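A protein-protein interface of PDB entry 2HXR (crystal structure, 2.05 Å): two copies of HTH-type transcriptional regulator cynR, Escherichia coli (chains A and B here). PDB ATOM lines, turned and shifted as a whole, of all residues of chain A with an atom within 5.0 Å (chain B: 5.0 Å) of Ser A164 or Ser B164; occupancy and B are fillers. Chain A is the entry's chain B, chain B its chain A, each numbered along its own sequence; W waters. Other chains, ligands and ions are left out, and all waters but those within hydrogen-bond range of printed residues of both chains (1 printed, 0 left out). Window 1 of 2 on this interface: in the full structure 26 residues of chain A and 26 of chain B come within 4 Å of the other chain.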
ATOM      1  N   THR A  41      13.136 -13.362 -26.655  1.00  0.00           N
ATOM      2  CA  THR A  41      14.026 -14.234 -25.911  1.00  0.00           C
ATOM      3  C   THR A  41      15.035 -13.394 -25.123  1.00  0.00           C
ATOM      4  O   THR A  41      15.420 -13.748 -24.015  1.00  0.00           O
ATOM      5  CB  THR A  41      14.814 -15.153 -26.861  1.00  0.00           C
ATOM      6  OG1 THR A  41      13.902 -15.896 -27.680  1.00  0.00           O
ATOM      7  CG2 THR A  41      15.687 -16.114 -26.064  1.00  0.00           C
ATOM      8  N   SER A 162      22.264 -14.606 -34.473  1.00  0.00           N
ATOM      9  CA  SER A 162      21.985 -14.717 -33.038  1.00  0.00           C
ATOM     10  C   SER A 162      22.035 -13.362 -32.310  1.00  0.00           C
ATOM     11  O   SER A 162      23.014 -12.626 -32.432  1.00  0.00           O
ATOM     12  CB  SER A 162      23.000 -15.680 -32.416  1.00  0.00           C
ATOM     13  OG  SER A 162      23.280 -15.364 -31.065  1.00  0.00           O
ATOM     14  N   ILE A 163      20.994 -13.029 -31.552  1.00  0.00           N
ATOM     15  CA  ILE A 163      20.992 -11.762 -30.821  1.00  0.00           C
ATOM     16  C   ILE A 163      22.106 -11.760 -29.776  1.00  0.00           C
ATOM     17  O   ILE A 163      22.782 -10.756 -29.596  1.00  0.00           O
ATOM     18  CB  ILE A 163      19.640 -11.481 -30.099  1.00  0.00           C
ATOM     19  CG1 ILE A 163      18.550 -11.114 -31.110  1.00  0.00           C
ATOM     20  CG2 ILE A 163      19.796 -10.313 -29.117  1.00  0.00           C
ATOM     21  CD1 ILE A 163      18.104 -12.259 -31.977  1.00  0.00           C
ATOM     22  N   SER A 164      22.298 -12.882 -29.086  1.00  0.00           N
ATOM     23  CA  SER A 164      23.349 -12.968 -28.077  1.00  0.00           C
ATOM     24  C   SER A 164      24.703 -12.604 -28.681  1.00  0.00           C
ATOM     25  O   SER A 164      25.445 -11.804 -28.118  1.00  0.00           O
ATOM     26  CB  SER A 164      23.446 -14.382 -27.498  1.00  0.00           C
ATOM     27  OG  SER A 164      22.192 -14.818 -27.036  1.00  0.00           O
ATOM     28  N   ALA A 165      25.028 -13.208 -29.816  1.00  0.00           N
ATOM     29  CA  ALA A 165      26.305 -12.925 -30.479  1.00  0.00           C
ATOM     30  C   ALA A 165      26.424 -11.429 -30.808  1.00  0.00           C
ATOM     31  O   ALA A 165      27.485 -10.815 -30.629  1.00  0.00           O
ATOM     32  CB  ALA A 165      26.432 -13.760 -31.769  1.00  0.00           C
ATOM     33  N   VAL A 166      25.336 -10.850 -31.302  1.00  0.00           N
ATOM     34  CA  VAL A 166      25.333  -9.433 -31.640  1.00  0.00           C
ATOM     35  C   VAL A 166      25.681  -8.615 -30.402  1.00  0.00           C
ATOM     36  O   VAL A 166      26.564  -7.757 -30.440  1.00  0.00           O
ATOM     37  CB  VAL A 166      23.950  -8.985 -32.166  1.00  0.00           C
ATOM     38  CG1 VAL A 166      23.929  -7.475 -32.386  1.00  0.00           C
ATOM     39  CG2 VAL A 166      23.645  -9.702 -33.458  1.00  0.00           C
ATOM     40  N   LEU A 167      24.986  -8.891 -29.306  1.00  0.00           N
ATOM     41  CA  LEU A 167      25.216  -8.171 -28.054  1.00  0.00           C
ATOM     42  C   LEU A 167      26.672  -8.275 -27.579  1.00  0.00           C
ATOM     43  O   LEU A 167      27.274  -7.289 -27.161  1.00  0.00           O
ATOM     44  CB  LEU A 167      24.271  -8.694 -26.959  1.00  0.00           C
ATOM     45  CG  LEU A 167      22.769  -8.529 -27.241  1.00  0.00           C
ATOM     46  CD1 LEU A 167      21.971  -8.920 -25.988  1.00  0.00           C
ATOM     47  CD2 LEU A 167      22.472  -7.090 -27.636  1.00  0.00           C
ATOM     48  N   GLU A 168      27.229  -9.477 -27.650  1.00  0.00           N
ATOM     49  CA  GLU A 168      28.602  -9.694 -27.228  1.00  0.00           C
ATOM     50  C   GLU A 168      29.550  -8.858 -28.092  1.00  0.00           C
ATOM     51  O   GLU A 168      30.496  -8.259 -27.589  1.00  0.00           O
ATOM     52  CB  GLU A 168      28.956 -11.179 -27.339  1.00  0.00           C
ATOM     53  CG  GLU A 168      30.282 -11.545 -26.689  1.00  0.00           C
ATOM     54  CD  GLU A 168      30.346 -11.117 -25.238  1.00  0.00           C
ATOM     55  OE1 GLU A 168      29.321 -11.262 -24.538  1.00  0.00           O
ATOM     56  OE2 GLU A 168      31.416 -10.643 -24.797  1.00  0.00           O
ATOM     57  N   ARG A 171      29.273  -5.158 -27.064  1.00  0.00           N
ATOM     58  CA  ARG A 171      29.912  -4.914 -25.772  1.00  0.00           C
ATOM     59  C   ARG A 171      31.420  -4.761 -25.922  1.00  0.00           C
ATOM     60  O   ARG A 171      32.031  -3.912 -25.279  1.00  0.00           O
ATOM     61  CB  ARG A 171      29.688  -6.074 -24.794  1.00  0.00           C
ATOM     62  CG  ARG A 171      28.270  -6.410 -24.404  1.00  0.00           C
ATOM     63  CD  ARG A 171      28.321  -7.305 -23.170  1.00  0.00           C
ATOM     64  NE  ARG A 171      27.014  -7.757 -22.702  1.00  0.00           N
ATOM     65  CZ  ARG A 171      26.377  -8.822 -23.178  1.00  0.00           C
ATOM     66  NH1 ARG A 171      26.925  -9.550 -24.145  1.00  0.00           N
ATOM     67  NH2 ARG A 171      25.202  -9.175 -22.672  1.00  0.00           N
ATOM     68  N   THR B  41      28.942 -19.887 -29.208  1.00  0.00           N
ATOM     69  CA  THR B  41      28.331 -18.568 -29.271  1.00  0.00           C
ATOM     70  C   THR B  41      28.297 -17.923 -27.890  1.00  0.00           C
ATOM     71  O   THR B  41      28.444 -16.712 -27.758  1.00  0.00           O
ATOM     72  CB  THR B  41      26.881 -18.666 -29.773  1.00  0.00           C
ATOM     73  OG1 THR B  41      26.862 -19.351 -31.034  1.00  0.00           O
ATOM     74  CG2 THR B  41      26.261 -17.268 -29.904  1.00  0.00           C
ATOM     75  N   SER B 162      17.295 -22.369 -26.670  1.00  0.00           N
ATOM     76  CA  SER B 162      18.220 -21.248 -26.634  1.00  0.00           C
ATOM     77  C   SER B 162      19.097 -21.248 -25.383  1.00  0.00           C
ATOM     78  O   SER B 162      18.588 -21.321 -24.264  1.00  0.00           O
ATOM     79  CB  SER B 162      17.447 -19.931 -26.673  1.00  0.00           C
ATOM     80  OG  SER B 162      18.215 -18.900 -26.073  1.00  0.00           O
ATOM     81  N   ILE B 163      20.407 -21.141 -25.564  1.00  0.00           N
ATOM     82  CA  ILE B 163      21.306 -21.099 -24.417  1.00  0.00           C
ATOM     83  C   ILE B 163      21.068 -19.816 -23.613  1.00  0.00           C
ATOM     84  O   ILE B 163      21.047 -19.850 -22.389  1.00  0.00           O
ATOM     85  CB  ILE B 163      22.798 -21.174 -24.844  1.00  0.00           C
ATOM     86  CG1 ILE B 163      23.162 -22.616 -25.206  1.00  0.00           C
ATOM     87  CG2 ILE B 163      23.706 -20.673 -23.717  1.00  0.00           C
ATOM     88  CD1 ILE B 163      24.642 -22.818 -25.545  1.00  0.00           C
ATOM     89  N   SER B 164      20.878 -18.690 -24.297  1.00  0.00           N
ATOM     90  CA  SER B 164      20.641 -17.436 -23.591  1.00  0.00           C
ATOM     91  C   SER B 164      19.373 -17.555 -22.738  1.00  0.00           C
ATOM     92  O   SER B 164      19.341 -17.081 -21.611  1.00  0.00           O
ATOM     93  CB  SER B 164      20.523 -16.257 -24.576  1.00  0.00           C
ATOM     94  OG  SER B 164      19.329 -16.318 -25.335  1.00  0.00           O
ATOM     95  N   ALA B 165      18.340 -18.205 -23.261  1.00  0.00           N
ATOM     96  CA  ALA B 165      17.105 -18.367 -22.495  1.00  0.00           C
ATOM     97  C   ALA B 165      17.348 -19.226 -21.248  1.00  0.00           C
ATOM     98  O   ALA B 165      16.813 -18.943 -20.177  1.00  0.00           O
ATOM     99  CB  ALA B 165      16.024 -18.995 -23.364  1.00  0.00           C
ATOM    100  N   VAL B 166      18.154 -20.276 -21.394  1.00  0.00           N
ATOM    101  CA  VAL B 166      18.469 -21.154 -20.269  1.00  0.00           C
ATOM    102  C   VAL B 166      19.203 -20.360 -19.192  1.00  0.00           C
ATOM    103  O   VAL B 166      18.851 -20.420 -18.024  1.00  0.00           O
ATOM    104  CB  VAL B 166      19.374 -22.350 -20.704  1.00  0.00           C
ATOM    105  CG1 VAL B 166      19.924 -23.065 -19.479  1.00  0.00           C
ATOM    106  CG2 VAL B 166      18.589 -23.334 -21.541  1.00  0.00           C
ATOM    107  N   LEU B 167      20.225 -19.612 -19.593  1.00  0.00           N
ATOM    108  CA  LEU B 167      20.999 -18.807 -18.651  1.00  0.00           C
ATOM    109  C   LEU B 167      20.127 -17.799 -17.893  1.00  0.00           C
ATOM    110  O   LEU B 167      20.312 -17.582 -16.692  1.00  0.00           O
ATOM    111  CB  LEU B 167      22.133 -18.078 -19.389  1.00  0.00           C
ATOM    112  CG  LEU B 167      23.209 -18.983 -20.034  1.00  0.00           C
ATOM    113  CD1 LEU B 167      24.350 -18.136 -20.620  1.00  0.00           C
ATOM    114  CD2 LEU B 167      23.770 -19.940 -18.993  1.00  0.00           C
ATOM    115  N   GLU B 168      19.177 -17.195 -18.600  1.00  0.00           N
ATOM    116  CA  GLU B 168      18.276 -16.213 -18.003  1.00  0.00           C
ATOM    117  C   GLU B 168      17.427 -16.882 -16.929  1.00  0.00           C
ATOM    118  O   GLU B 168      17.208 -16.333 -15.835  1.00  0.00           O
ATOM    119  CB  GLU B 168      17.356 -15.637 -19.074  1.00  0.00           C
ATOM    120  CG  GLU B 168      16.400 -14.607 -18.552  1.00  0.00           C
ATOM    121  CD  GLU B 168      16.886 -13.222 -18.843  1.00  0.00           C
ATOM    122  OE1 GLU B 168      16.581 -12.706 -19.949  1.00  0.00           O
ATOM    123  OE2 GLU B 168      17.589 -12.666 -17.972  1.00  0.00           O
ATOM    124  N   ARG B 171      19.544 -17.707 -13.791  1.00  0.00           N
ATOM    125  CA  ARG B 171      19.869 -16.577 -12.934  1.00  0.00           C
ATOM    126  C   ARG B 171      18.676 -16.101 -12.127  1.00  0.00           C
ATOM    127  O   ARG B 171      18.840 -15.595 -11.019  1.00  0.00           O
ATOM    128  CB  ARG B 171      20.486 -15.388 -13.706  1.00  0.00           C
ATOM    129  CG  ARG B 171      19.957 -15.042 -15.085  1.00  0.00           C
ATOM    130  CD  ARG B 171      20.619 -13.728 -15.568  1.00  0.00           C
ATOM    131  NE  ARG B 171      20.627 -13.575 -17.029  1.00  0.00           N
ATOM    132  CZ  ARG B 171      21.562 -14.082 -17.835  1.00  0.00           C
ATOM    133  NH1 ARG B 171      22.576 -14.771 -17.331  1.00  0.00           N
ATOM    134  NH2 ARG B 171      21.482 -13.912 -19.145  1.00  0.00           N
HETATM  135  O   HOH W   1      14.289 -12.536 -21.525  1.00  0.00           O
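The side-chain hydroxyl (OG) of Ser B164 sits at hydrogen-bond distance from the side-chain hydroxyl (OG) of Ser B162. N of Ala B165 is in hydrogen-bond range of OG of Ser B162, at 2.9 Å. The side-chain hydroxyl (OG) of Ser A162 sits close to the backbone NH (N) of Ser A164, 3.3 Å away. OG of Ser A162 sits at hydrogen-bond distance from N of Ala A165.
Ser B162 touches Thr A41. Thr A41 touches Ser B164. Ala B165 touches Thr A41 (CB to CG2, 3.96 Å). OG of Ser A162 touches CG2 of Thr B41 (3.7 Å). Ser A164 touches Ser B164. CB of Ala A165 touches CG2 of Thr B41, at 3.98 Å.
Of chain B, only Ser B164 comes within 4 Å of Ser A164. Ser B164 touches just these residues of chain A: Thr A41 and Ser A164. Of the printed residues of chain A, Thr B41 touches Ser A162 and Ala A165. Printed residues of chain A within 4 Å of Ala B165: Thr A41. Printed residues of chain A within 4 Å of Ser B162: Thr A41 (3.8 Å). Of the printed residues of chain B, Ala A165 touches Thr B41. Glu A168 touches none of the printed residues of chain B. Ile A163 touches none of the printed residues of chain B.
Hydrophobic or aromatic side chains of chain A that line the printed part of chain B: Ala A165. Of the 9 printed residues of chain B, 4 touch a printed residue of chain A. Among the printed residues, no Asp or Glu carboxylate lies within 4 Å of a Lys or Arg side-chain nitrogen of the other chain.
Thr A41 touches Ser B162, and with the chains exchanged Ser A162 touches Thr B41. Thr A41 touches Ser B164, but with the chains exchanged Ser A164 does not touch Thr B41 (4.7 Å). Thr A41 touches Ala B165, and with the chains exchanged Ala A165 touches Thr B41. Ser B164 touches its own counterpart, Ser A164. Positions printed for both chains: 41, 162, 163, 164, 165, 166, 167, 168 and 171. Of the 6 pairs that touch across the chains among the printed residues, 5 have their exchanged pair printed and touching as well.
Water W1 lies within hydrogen-bond range of OE1 of Glu B168 (2.8 Å) and O of Thr A41 (3.0 Å).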
